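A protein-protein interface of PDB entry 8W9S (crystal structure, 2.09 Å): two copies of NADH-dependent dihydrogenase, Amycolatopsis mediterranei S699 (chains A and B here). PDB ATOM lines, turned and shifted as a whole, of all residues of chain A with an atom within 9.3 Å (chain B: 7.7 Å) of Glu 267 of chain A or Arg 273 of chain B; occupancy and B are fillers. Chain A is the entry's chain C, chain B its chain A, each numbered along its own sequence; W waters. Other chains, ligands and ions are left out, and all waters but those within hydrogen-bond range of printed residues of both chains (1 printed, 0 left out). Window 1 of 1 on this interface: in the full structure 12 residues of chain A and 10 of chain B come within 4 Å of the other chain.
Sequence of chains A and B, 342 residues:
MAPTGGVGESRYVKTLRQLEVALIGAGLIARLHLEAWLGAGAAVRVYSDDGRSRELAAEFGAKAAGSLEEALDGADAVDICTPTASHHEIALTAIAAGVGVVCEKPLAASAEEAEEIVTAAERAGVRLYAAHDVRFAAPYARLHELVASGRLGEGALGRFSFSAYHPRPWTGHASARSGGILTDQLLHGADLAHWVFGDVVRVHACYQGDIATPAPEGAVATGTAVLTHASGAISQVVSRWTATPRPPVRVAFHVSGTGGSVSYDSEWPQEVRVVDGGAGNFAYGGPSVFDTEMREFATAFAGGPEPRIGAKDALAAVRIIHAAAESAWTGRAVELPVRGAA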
ATOM      1  N   TYR A 140     -18.695  13.443 -15.102  1.00  0.00           N
ATOM      2  CA  TYR A 140     -19.693  12.647 -15.808  1.00  0.00           C
ATOM      3  C   TYR A 140     -21.080  13.253 -15.641  1.00  0.00           C
ATOM      4  O   TYR A 140     -21.867  13.280 -16.590  1.00  0.00           O
ATOM      5  CB  TYR A 140     -19.637  11.205 -15.297  1.00  0.00           C
ATOM      6  CG  TYR A 140     -18.197  10.798 -15.015  1.00  0.00           C
ATOM      7  CD1 TYR A 140     -17.318  10.530 -16.063  1.00  0.00           C
ATOM      8  CD2 TYR A 140     -17.708  10.741 -13.718  1.00  0.00           C
ATOM      9  CE1 TYR A 140     -15.972  10.191 -15.817  1.00  0.00           C
ATOM     10  CE2 TYR A 140     -16.363  10.400 -13.455  1.00  0.00           C
ATOM     11  CZ  TYR A 140     -15.507  10.131 -14.514  1.00  0.00           C
ATOM     12  OH  TYR A 140     -14.193   9.803 -14.274  1.00  0.00           O
ATOM     13  N   ARG A 159     -16.138   8.032 -27.071  1.00  0.00           N
ATOM     14  CA  ARG A 159     -15.187   7.051 -26.570  1.00  0.00           C
ATOM     15  C   ARG A 159     -15.019   7.264 -25.076  1.00  0.00           C
ATOM     16  O   ARG A 159     -14.971   8.407 -24.602  1.00  0.00           O
ATOM     17  CB  ARG A 159     -13.847   7.114 -27.307  1.00  0.00           C
ATOM     18  CG  ARG A 159     -13.090   8.417 -27.219  1.00  0.00           C
ATOM     19  CD  ARG A 159     -11.660   8.213 -27.755  1.00  0.00           C
ATOM     20  NE  ARG A 159     -11.012   9.493 -28.004  1.00  0.00           N
ATOM     21  CZ  ARG A 159     -10.427  10.222 -27.058  1.00  0.00           C
ATOM     22  NH1 ARG A 159     -10.399   9.802 -25.792  1.00  0.00           N
ATOM     23  NH2 ARG A 159      -9.875  11.384 -27.374  1.00  0.00           N
ATOM     24  N   SER A 163      -9.452   2.926 -16.569  1.00  0.00           N
ATOM     25  CA  SER A 163      -8.239   2.158 -16.305  1.00  0.00           C
ATOM     26  C   SER A 163      -7.806   2.369 -14.867  1.00  0.00           C
ATOM     27  O   SER A 163      -7.734   3.513 -14.399  1.00  0.00           O
ATOM     28  CB  SER A 163      -7.069   2.561 -17.221  1.00  0.00           C
ATOM     29  OG  SER A 163      -7.450   2.648 -18.581  1.00  0.00           O
ATOM     30  N   PRO A 245       0.358   1.011 -10.123  1.00  0.00           N
ATOM     31  CA  PRO A 245      -0.421   2.238  -9.836  1.00  0.00           C
ATOM     32  C   PRO A 245       0.233   3.510 -10.380  1.00  0.00           C
ATOM     33  O   PRO A 245       0.437   4.476  -9.646  1.00  0.00           O
ATOM     34  CB  PRO A 245      -0.491   2.244  -8.314  1.00  0.00           C
ATOM     35  CG  PRO A 245       0.789   1.552  -7.878  1.00  0.00           C
ATOM     36  CD  PRO A 245       1.032   0.490  -8.919  1.00  0.00           C
ATOM     37  N   ARG A 246       0.565   3.515 -11.666  1.00  0.00           N
ATOM     38  CA  ARG A 246       1.280   4.621 -12.308  1.00  0.00           C
ATOM     39  C   ARG A 246       0.497   5.116 -13.518  1.00  0.00           C
ATOM     40  O   ARG A 246       0.942   4.963 -14.658  1.00  0.00           O
ATOM     41  CB  ARG A 246       2.689   4.197 -12.735  1.00  0.00           C
ATOM     42  CG  ARG A 246       3.571   3.639 -11.625  1.00  0.00           C
ATOM     43  CD  ARG A 246       5.060   3.648 -12.019  1.00  0.00           C
ATOM     44  NE  ARG A 246       5.702   4.927 -11.690  1.00  0.00           N
ATOM     45  CZ  ARG A 246       7.013   5.159 -11.733  1.00  0.00           C
ATOM     46  NH1 ARG A 246       7.860   4.198 -12.089  1.00  0.00           N
ATOM     47  NH2 ARG A 246       7.482   6.359 -11.406  1.00  0.00           N
ATOM     48  N   PRO A 247      -0.665   5.759 -13.306  1.00  0.00           N
ATOM     49  CA  PRO A 247      -1.286   6.181 -12.048  1.00  0.00           C
ATOM     50  C   PRO A 247      -2.233   5.124 -11.476  1.00  0.00           C
ATOM     51  O   PRO A 247      -2.497   4.138 -12.146  1.00  0.00           O
ATOM     52  CB  PRO A 247      -2.058   7.443 -12.461  1.00  0.00           C
ATOM     53  CG  PRO A 247      -2.510   7.138 -13.863  1.00  0.00           C
ATOM     54  CD  PRO A 247      -1.472   6.174 -14.469  1.00  0.00           C
ATOM     55  N   PRO A 248      -2.708   5.321 -10.243  1.00  0.00           N
ATOM     56  CA  PRO A 248      -3.675   4.362  -9.677  1.00  0.00           C
ATOM     57  C   PRO A 248      -4.967   4.226 -10.485  1.00  0.00           C
ATOM     58  O   PRO A 248      -5.527   3.121 -10.547  1.00  0.00           O
ATOM     59  CB  PRO A 248      -3.956   4.917  -8.268  1.00  0.00           C
ATOM     60  CG  PRO A 248      -2.963   6.027  -8.028  1.00  0.00           C
ATOM     61  CD  PRO A 248      -2.099   6.200  -9.227  1.00  0.00           C
ATOM     62  N   VAL A 249      -5.459   5.314 -11.084  1.00  0.00           N
ATOM     63  CA  VAL A 249      -6.706   5.337 -11.862  1.00  0.00           C
ATOM     64  C   VAL A 249      -6.567   6.399 -12.948  1.00  0.00           C
ATOM     65  O   VAL A 249      -6.008   7.474 -12.709  1.00  0.00           O
ATOM     66  CB  VAL A 249      -7.951   5.640 -10.977  1.00  0.00           C
ATOM     67  CG1 VAL A 249      -8.265   4.528  -9.969  1.00  0.00           C
ATOM     68  CG2 VAL A 249      -7.764   6.938 -10.211  1.00  0.00           C
ATOM     69  N   ARG A 250      -7.054   6.102 -14.153  1.00  0.00           N
ATOM     70  CA  ARG A 250      -7.196   7.127 -15.183  1.00  0.00           C
ATOM     71  C   ARG A 250      -8.515   6.911 -15.902  1.00  0.00           C
ATOM     72  O   ARG A 250      -8.819   5.782 -16.305  1.00  0.00           O
ATOM     73  CB  ARG A 250      -6.055   7.119 -16.217  1.00  0.00           C
ATOM     74  CG  ARG A 250      -6.337   8.077 -17.380  1.00  0.00           C
ATOM     75  CD  ARG A 250      -5.129   8.395 -18.240  1.00  0.00           C
ATOM     76  NE  ARG A 250      -5.430   9.414 -19.255  1.00  0.00           N
ATOM     77  CZ  ARG A 250      -5.786   9.143 -20.513  1.00  0.00           C
ATOM     78  NH1 ARG A 250      -5.901   7.881 -20.906  1.00  0.00           N
ATOM     79  NH2 ARG A 250      -6.059  10.130 -21.369  1.00  0.00           N
ATOM     80  N   VAL A 251      -9.295   7.981 -16.049  1.00  0.00           N
ATOM     81  CA  VAL A 251     -10.541   7.961 -16.815  1.00  0.00           C
ATOM     82  C   VAL A 251     -10.448   9.032 -17.891  1.00  0.00           C
ATOM     83  O   VAL A 251     -10.024  10.161 -17.611  1.00  0.00           O
ATOM     84  CB  VAL A 251     -11.776   8.194 -15.918  1.00  0.00           C
ATOM     85  CG1 VAL A 251     -13.075   8.192 -16.755  1.00  0.00           C
ATOM     86  CG2 VAL A 251     -11.833   7.146 -14.811  1.00  0.00           C
ATOM     87  N   ALA A 252     -10.842   8.684 -19.122  1.00  0.00           N
ATOM     88  CA  ALA A 252     -10.851   9.647 -20.209  1.00  0.00           C
ATOM     89  C   ALA A 252     -12.078   9.423 -21.078  1.00  0.00           C
ATOM     90  O   ALA A 252     -12.525   8.286 -21.263  1.00  0.00           O
ATOM     91  CB  ALA A 252      -9.580   9.549 -21.065  1.00  0.00           C
ATOM     92  N   PHE A 253     -12.630  10.517 -21.609  1.00  0.00           N
ATOM     93  CA  PHE A 253     -13.701  10.362 -22.583  1.00  0.00           C
ATOM     94  C   PHE A 253     -13.691  11.520 -23.570  1.00  0.00           C
ATOM     95  O   PHE A 253     -13.117  12.582 -23.313  1.00  0.00           O
ATOM     96  CB  PHE A 253     -15.080  10.190 -21.900  1.00  0.00           C
ATOM     97  CG  PHE A 253     -15.595  11.420 -21.123  1.00  0.00           C
ATOM     98  CD1 PHE A 253     -15.947  12.596 -21.779  1.00  0.00           C
ATOM     99  CD2 PHE A 253     -15.797  11.347 -19.739  1.00  0.00           C
ATOM    100  CE1 PHE A 253     -16.463  13.693 -21.074  1.00  0.00           C
ATOM    101  CE2 PHE A 253     -16.306  12.442 -19.017  1.00  0.00           C
ATOM    102  CZ  PHE A 253     -16.635  13.612 -19.689  1.00  0.00           C
ATOM    103  N   TYR A 264     -12.680  14.883 -21.579  1.00  0.00           N
ATOM    104  CA  TYR A 264     -12.223  14.816 -20.196  1.00  0.00           C
ATOM    105  C   TYR A 264     -11.012  13.898 -20.071  1.00  0.00           C
ATOM    106  O   TYR A 264     -10.962  12.827 -20.687  1.00  0.00           O
ATOM    107  CB  TYR A 264     -13.341  14.324 -19.269  1.00  0.00           C
ATOM    108  CG  TYR A 264     -12.903  14.049 -17.846  1.00  0.00           C
ATOM    109  CD1 TYR A 264     -12.512  15.086 -16.994  1.00  0.00           C
ATOM    110  CD2 TYR A 264     -12.894  12.761 -17.348  1.00  0.00           C
ATOM    111  CE1 TYR A 264     -12.125  14.832 -15.692  1.00  0.00           C
ATOM    112  CE2 TYR A 264     -12.519  12.494 -16.061  1.00  0.00           C
ATOM    113  CZ  TYR A 264     -12.121  13.525 -15.234  1.00  0.00           C
ATOM    114  OH  TYR A 264     -11.735  13.233 -13.947  1.00  0.00           O
ATOM    115  N   ASP A 265     -10.049  14.308 -19.246  1.00  0.00           N
ATOM    116  CA  ASP A 265      -8.926  13.451 -18.865  1.00  0.00           C
ATOM    117  C   ASP A 265      -8.703  13.656 -17.375  1.00  0.00           C
ATOM    118  O   ASP A 265      -8.437  14.779 -16.946  1.00  0.00           O
ATOM    119  CB  ASP A 265      -7.666  13.804 -19.668  1.00  0.00           C
ATOM    120  CG  ASP A 265      -6.527  12.768 -19.529  1.00  0.00           C
ATOM    121  OD1 ASP A 265      -6.439  12.000 -18.532  1.00  0.00           O
ATOM    122  OD2 ASP A 265      -5.677  12.759 -20.449  1.00  0.00           O
ATOM    123  N   SER A 266      -8.843  12.583 -16.587  1.00  0.00           N
ATOM    124  CA  SER A 266      -8.647  12.690 -15.152  1.00  0.00           C
ATOM    125  C   SER A 266      -7.217  13.087 -14.786  1.00  0.00           C
ATOM    126  O   SER A 266      -6.983  13.476 -13.641  1.00  0.00           O
ATOM    127  CB  SER A 266      -9.030  11.376 -14.466  1.00  0.00           C
ATOM    128  OG  SER A 266      -8.232  10.294 -14.928  1.00  0.00           O
ATOM    129  N   GLU A 267      -6.272  13.018 -15.732  1.00  0.00           N
ATOM    130  CA  GLU A 267      -4.890  13.445 -15.500  1.00  0.00           C
ATOM    131  C   GLU A 267      -4.726  14.958 -15.584  1.00  0.00           C
ATOM    132  O   GLU A 267      -3.700  15.482 -15.144  1.00  0.00           O
ATOM    133  CB  GLU A 267      -3.945  12.800 -16.527  1.00  0.00           C
ATOM    134  CG  GLU A 267      -3.785  11.281 -16.397  1.00  0.00           C
ATOM    135  CD  GLU A 267      -2.925  10.897 -15.203  1.00  0.00           C
ATOM    136  OE1 GLU A 267      -1.703  10.689 -15.395  1.00  0.00           O
ATOM    137  OE2 GLU A 267      -3.464  10.791 -14.081  1.00  0.00           O
ATOM    138  N   TRP A 268      -5.678  15.665 -16.176  1.00  0.00           N
ATOM    139  CA  TRP A 268      -5.607  17.122 -16.184  1.00  0.00           C
ATOM    140  C   TRP A 268      -5.554  17.633 -14.745  1.00  0.00           C
ATOM    141  O   TRP A 268      -6.238  17.086 -13.877  1.00  0.00           O
ATOM    142  CB  TRP A 268      -6.832  17.720 -16.885  1.00  0.00           C
ATOM    143  CG  TRP A 268      -6.926  17.504 -18.376  1.00  0.00           C
ATOM    144  CD1 TRP A 268      -5.900  17.204 -19.255  1.00  0.00           C
ATOM    145  CD2 TRP A 268      -8.121  17.596 -19.168  1.00  0.00           C
ATOM    146  NE1 TRP A 268      -6.401  17.095 -20.541  1.00  0.00           N
ATOM    147  CE2 TRP A 268      -7.756  17.339 -20.515  1.00  0.00           C
ATOM    148  CE3 TRP A 268      -9.466  17.861 -18.867  1.00  0.00           C
ATOM    149  CZ2 TRP A 268      -8.689  17.353 -21.556  1.00  0.00           C
ATOM    150  CZ3 TRP A 268     -10.392  17.877 -19.906  1.00  0.00           C
ATOM    151  CH2 TRP A 268      -9.999  17.625 -21.231  1.00  0.00           C
ATOM    152  N   PRO A 269      -4.752  18.662 -14.453  1.00  0.00           N
ATOM    153  CA  PRO A 269      -4.797  19.269 -13.113  1.00  0.00           C
ATOM    154  C   PRO A 269      -6.158  19.892 -12.839  1.00  0.00           C
ATOM    155  O   PRO A 269      -6.792  20.462 -13.729  1.00  0.00           O
ATOM    156  CB  PRO A 269      -3.703  20.345 -13.168  1.00  0.00           C
ATOM    157  CG  PRO A 269      -3.560  20.660 -14.647  1.00  0.00           C
ATOM    158  CD  PRO A 269      -3.740  19.303 -15.311  1.00  0.00           C
ATOM    159  N   GLN A 270      -6.598  19.789 -11.596  1.00  0.00           N
ATOM    160  CA  GLN A 270      -7.843  20.413 -11.141  1.00  0.00           C
ATOM    161  C   GLN A 270      -7.496  21.502 -10.139  1.00  0.00           C
ATOM    162  O   GLN A 270      -6.584  22.297 -10.416  1.00  0.00           O
ATOM    163  CB  GLN A 270      -8.783  19.320 -10.646  1.00  0.00           C
ATOM    164  CG  GLN A 270      -9.337  18.430 -11.770  1.00  0.00           C
ATOM    165  CD  GLN A 270     -10.069  19.235 -12.836  1.00  0.00           C
ATOM    166  OE1 GLN A 270     -10.823  20.170 -12.521  1.00  0.00           O
ATOM    167  NE2 GLN A 270      -9.891  18.857 -14.089  1.00  0.00           N
ATOM    168  N   VAL A 272      -5.938  21.473  -7.144  1.00  0.00           N
ATOM    169  CA  VAL A 272      -4.645  21.355  -6.454  1.00  0.00           C
ATOM    170  C   VAL A 272      -3.640  20.690  -7.387  1.00  0.00           C
ATOM    171  O   VAL A 272      -3.867  19.570  -7.857  1.00  0.00           O
ATOM    172  CB  VAL A 272      -4.768  20.560  -5.147  1.00  0.00           C
ATOM    173  CG1 VAL A 272      -3.430  20.577  -4.372  1.00  0.00           C
ATOM    174  CG2 VAL A 272      -5.888  21.142  -4.292  1.00  0.00           C
ATOM    175  N   ARG A 273      -2.515  21.357  -7.635  1.00  0.00           N
ATOM    176  CA  ARG A 273      -1.524  20.811  -8.560  1.00  0.00           C
ATOM    177  C   ARG A 273      -0.124  21.103  -8.043  1.00  0.00           C
ATOM    178  O   ARG A 273       0.262  22.276  -7.930  1.00  0.00           O
ATOM    179  CB  ARG A 273      -1.705  21.406  -9.954  1.00  0.00           C
ATOM    180  CG  ARG A 273      -0.597  21.059 -10.943  1.00  0.00           C
ATOM    181  CD  ARG A 273      -0.702  21.957 -12.177  1.00  0.00           C
ATOM    182  NE  ARG A 273       0.367  21.727 -13.157  1.00  0.00           N
ATOM    183  CZ  ARG A 273       0.530  22.454 -14.259  1.00  0.00           C
ATOM    184  NH1 ARG A 273       1.539  22.184 -15.076  1.00  0.00           N
ATOM    185  NH2 ARG A 273      -0.304  23.464 -14.531  1.00  0.00           N
ATOM    186  N   TRP B 268       2.408  20.186 -20.808  1.00  0.00           N
ATOM    187  CA  TRP B 268       1.338  19.551 -21.576  1.00  0.00           C
ATOM    188  C   TRP B 268       1.936  18.448 -22.448  1.00  0.00           C
ATOM    189  O   TRP B 268       3.048  18.611 -22.968  1.00  0.00           O
ATOM    190  CB  TRP B 268       0.622  20.553 -22.492  1.00  0.00           C
ATOM    191  CG  TRP B 268      -0.208  21.610 -21.846  1.00  0.00           C
ATOM    192  CD1 TRP B 268      -0.765  21.579 -20.598  1.00  0.00           C
ATOM    193  CD2 TRP B 268      -0.590  22.875 -22.429  1.00  0.00           C
ATOM    194  NE1 TRP B 268      -1.463  22.746 -20.369  1.00  0.00           N
ATOM    195  CE2 TRP B 268      -1.366  23.557 -21.472  1.00  0.00           C
ATOM    196  CE3 TRP B 268      -0.348  23.490 -23.674  1.00  0.00           C
ATOM    197  CZ2 TRP B 268      -1.921  24.828 -21.716  1.00  0.00           C
ATOM    198  CZ3 TRP B 268      -0.887  24.750 -23.915  1.00  0.00           C
ATOM    199  CH2 TRP B 268      -1.671  25.409 -22.934  1.00  0.00           C
ATOM    200  N   PRO B 269       1.222  17.338 -22.656  1.00  0.00           N
ATOM    201  CA  PRO B 269       1.734  16.289 -23.558  1.00  0.00           C
ATOM    202  C   PRO B 269       1.749  16.764 -25.004  1.00  0.00           C
ATOM    203  O   PRO B 269       0.862  17.496 -25.446  1.00  0.00           O
ATOM    204  CB  PRO B 269       0.735  15.141 -23.362  1.00  0.00           C
ATOM    205  CG  PRO B 269      -0.572  15.874 -23.021  1.00  0.00           C
ATOM    206  CD  PRO B 269      -0.113  17.007 -22.115  1.00  0.00           C
ATOM    207  N   GLN B 270       2.765  16.344 -25.749  1.00  0.00           N
ATOM    208  CA  GLN B 270       2.816  16.690 -27.167  1.00  0.00           C
ATOM    209  C   GLN B 270       2.709  15.421 -28.028  1.00  0.00           C
ATOM    210  O   GLN B 270       1.742  14.661 -27.875  1.00  0.00           O
ATOM    211  CB  GLN B 270       4.079  17.509 -27.450  1.00  0.00           C
ATOM    212  CG  GLN B 270       4.022  18.939 -26.839  1.00  0.00           C
ATOM    213  CD  GLN B 270       2.889  19.781 -27.393  1.00  0.00           C
ATOM    214  OE1 GLN B 270       2.567  19.688 -28.575  1.00  0.00           O
ATOM    215  NE2 GLN B 270       2.290  20.628 -26.546  1.00  0.00           N
ATOM    216  N   GLU B 271       3.680  15.162 -28.919  1.00  0.00           N
ATOM    217  CA  GLU B 271       3.513  14.060 -29.872  1.00  0.00           C
ATOM    218  C   GLU B 271       3.668  12.694 -29.222  1.00  0.00           C
ATOM    219  O   GLU B 271       3.034  11.732 -29.672  1.00  0.00           O
ATOM    220  CB  GLU B 271       4.508  14.159 -31.027  1.00  0.00           C
ATOM    221  CG  GLU B 271       4.296  15.348 -31.930  1.00  0.00           C
ATOM    222  CD  GLU B 271       5.065  16.566 -31.428  1.00  0.00           C
ATOM    223  OE1 GLU B 271       5.591  16.503 -30.296  1.00  0.00           O
ATOM    224  OE2 GLU B 271       5.129  17.581 -32.155  1.00  0.00           O
ATOM    225  N   VAL B 272       4.501  12.573 -28.190  1.00  0.00           N
ATOM    226  CA  VAL B 272       4.782  11.292 -27.559  1.00  0.00           C
ATOM    227  C   VAL B 272       4.418  11.396 -26.093  1.00  0.00           C
ATOM    228  O   VAL B 272       4.999  12.214 -25.369  1.00  0.00           O
ATOM    229  CB  VAL B 272       6.257  10.887 -27.699  1.00  0.00           C
ATOM    230  CG1 VAL B 272       6.509   9.608 -26.920  1.00  0.00           C
ATOM    231  CG2 VAL B 272       6.648  10.764 -29.174  1.00  0.00           C
ATOM    232  N   ARG B 273       3.518  10.525 -25.637  1.00  0.00           N
ATOM    233  CA  ARG B 273       3.033  10.590 -24.262  1.00  0.00           C
ATOM    234  C   ARG B 273       2.908   9.190 -23.677  1.00  0.00           C
ATOM    235  O   ARG B 273       2.117   8.373 -24.166  1.00  0.00           O
ATOM    236  CB  ARG B 273       1.685  11.320 -24.205  1.00  0.00           C
ATOM    237  CG  ARG B 273       1.078  11.401 -22.815  1.00  0.00           C
ATOM    238  CD  ARG B 273      -0.425  11.757 -22.920  1.00  0.00           C
ATOM    239  NE  ARG B 273      -1.093  11.725 -21.621  1.00  0.00           N
ATOM    240  CZ  ARG B 273      -2.375  12.018 -21.435  1.00  0.00           C
ATOM    241  NH1 ARG B 273      -3.129  12.369 -22.471  1.00  0.00           N
ATOM    242  NH2 ARG B 273      -2.894  11.953 -20.217  1.00  0.00           N
ATOM    243  N   VAL B 274       3.682   8.918 -22.630  1.00  0.00           N
ATOM    244  CA  VAL B 274       3.511   7.699 -21.847  1.00  0.00           C
ATOM    245  C   VAL B 274       2.301   7.922 -20.948  1.00  0.00           C
ATOM    246  O   VAL B 274       2.308   8.805 -20.089  1.00  0.00           O
ATOM    247  CB  VAL B 274       4.758   7.364 -21.025  1.00  0.00           C
ATOM    248  CG1 VAL B 274       4.528   6.098 -20.215  1.00  0.00           C
ATOM    249  CG2 VAL B 274       5.982   7.218 -21.924  1.00  0.00           C
ATOM    250  N   VAL B 275       1.248   7.144 -21.161  1.00  0.00           N
ATOM    251  CA  VAL B 275       0.015   7.388 -20.421  1.00  0.00           C
ATOM    252  C   VAL B 275       0.022   6.657 -19.088  1.00  0.00           C
ATOM    253  O   VAL B 275      -0.412   7.212 -18.079  1.00  0.00           O
ATOM    254  CB  VAL B 275      -1.208   7.019 -21.288  1.00  0.00           C
ATOM    255  CG1 VAL B 275      -2.509   7.232 -20.513  1.00  0.00           C
ATOM    256  CG2 VAL B 275      -1.218   7.875 -22.539  1.00  0.00           C
ATOM    257  N   ASP B 276       0.550   5.431 -19.040  1.00  0.00           N
ATOM    258  CA  ASP B 276       0.648   4.713 -17.776  1.00  0.00           C
ATOM    259  C   ASP B 276       1.824   3.746 -17.798  1.00  0.00           C
ATOM    260  O   ASP B 276       2.367   3.417 -18.855  1.00  0.00           O
ATOM    261  CB  ASP B 276      -0.641   3.959 -17.467  1.00  0.00           C
ATOM    262  CG  ASP B 276      -1.086   3.086 -18.616  1.00  0.00           C
ATOM    263  OD1 ASP B 276      -0.699   1.902 -18.639  1.00  0.00           O
ATOM    264  OD2 ASP B 276      -1.813   3.594 -19.506  1.00  0.00           O
ATOM    265  N   PHE B 282      10.904   6.643 -23.965  1.00  0.00           N
ATOM    266  CA  PHE B 282      10.111   7.306 -24.997  1.00  0.00           C
ATOM    267  C   PHE B 282      10.400   8.803 -25.052  1.00  0.00           C
ATOM    268  O   PHE B 282       9.519   9.608 -25.375  1.00  0.00           O
ATOM    269  CB  PHE B 282       8.620   7.056 -24.784  1.00  0.00           C
ATOM    270  CG  PHE B 282       8.212   5.636 -25.021  1.00  0.00           C
ATOM    271  CD1 PHE B 282       8.032   4.767 -23.953  1.00  0.00           C
ATOM    272  CD2 PHE B 282       8.009   5.163 -26.308  1.00  0.00           C
ATOM    273  CE1 PHE B 282       7.646   3.444 -24.169  1.00  0.00           C
ATOM    274  CE2 PHE B 282       7.619   3.851 -26.529  1.00  0.00           C
ATOM    275  CZ  PHE B 282       7.443   2.986 -25.458  1.00  0.00           C
ATOM    276  N   TYR B 284      11.228  12.314 -26.290  1.00  0.00           N
ATOM    277  CA  TYR B 284      11.131  13.022 -27.560  1.00  0.00           C
ATOM    278  C   TYR B 284      10.900  14.489 -27.257  1.00  0.00           C
ATOM    279  O   TYR B 284       9.954  14.828 -26.539  1.00  0.00           O
ATOM    280  CB  TYR B 284       9.999  12.484 -28.441  1.00  0.00           C
ATOM    281  CG  TYR B 284       9.756  13.326 -29.672  1.00  0.00           C
ATOM    282  CD1 TYR B 284      10.615  13.255 -30.759  1.00  0.00           C
ATOM    283  CD2 TYR B 284       8.691  14.207 -29.742  1.00  0.00           C
ATOM    284  CE1 TYR B 284      10.412  14.034 -31.887  1.00  0.00           C
ATOM    285  CE2 TYR B 284       8.473  14.982 -30.862  1.00  0.00           C
ATOM    286  CZ  TYR B 284       9.342  14.890 -31.936  1.00  0.00           C
ATOM    287  OH  TYR B 284       9.148  15.657 -33.064  1.00  0.00           O
HETATM  288  O   HOH W   1      -1.463   9.770 -17.850  1.00  0.00           O
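Printed residues of chain A that touch a printed residue of chain B: Arg 246, Pro 247, Arg 250, Asp 265 and Glu 267. Of the 11 printed residues of chain B, 3 touch a printed residue of chain A. Hydrophobic or aromatic side chains of chain B that line the printed part of chain A: Val 275. Among the printed residues, 7 pairs touch across the chains. Among the printed residues, Asp or Glu carboxylates within 4 Å of a Lys or Arg side-chain nitrogen of the other chain: Asp 265 of chain A with Arg 273 of chain B.
Among the printed residues, merely in contact across the chains: Arg 246 of chain A with Asp 276 of chain B (3.1 Å), Pro 247 of chain A with Val 275 of chain B (3.9 Å), Pro 247 of chain A with Asp 276 of chain B (3.8 Å), Arg 250 of chain A with Arg 273 of chain B (3.7 Å), Arg 250 of chain A with Val 275 of chain B (3.5 Å) and Glu 267 of chain A with Arg 273 of chain B (3.9 Å).
Of the printed residues of chain B, Glu 267 of chain A touches Arg 273 (3.9 Å). Of chain A, only Arg 250, Asp 265 and Glu 267 come within 4 Å of Arg 273 of chain B. Ser 266 of chain A touches none of the printed residues of chain B. No residue of chain A comes within 4 Å of Val 272 of chain B. No residue of chain A comes within 4 Å of Val 274 of chain B. Printed residues of chain B within 4 Å of Arg 250 of chain A: Arg 273 and Val 275. Of the printed residues of chain B, Pro 247 of chain A touches Val 275 (3.9 Å) and Asp 276 (3.8 Å). The nearest residue of chain B that does not touch Glu 267 of chain A is Val 275 of chain B (4.6 Å).
5 positions are printed for both chains. Of the 7 pairs that touch across the chains among the printed residues, none has its exchanged pair printed and touching as well.
The guanidinium group of Arg 250 of chain A lies within salt-bridge range of the side-chain carboxylate of Asp 265 of chain A (2.8 Å). OD1 of Asp 265 of chain A sits at hydrogen-bond distance from N of Glu 267 of chain A (3.0 Å). The backbone carbonyl oxygen (O) of Ser 163 of chain A sits at hydrogen-bond distance from the backbone NH (N) of Arg 250 of chain A (2.7 Å).
Water W1 bridges OE1 of Glu 267 of chain A (2.6 Å) and O of Val 275 of chain B (2.8 Å).
NH2 of Arg 273 of chain B is in salt-bridge range of OD2 of Asp 265 of chain A (2.9 Å).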
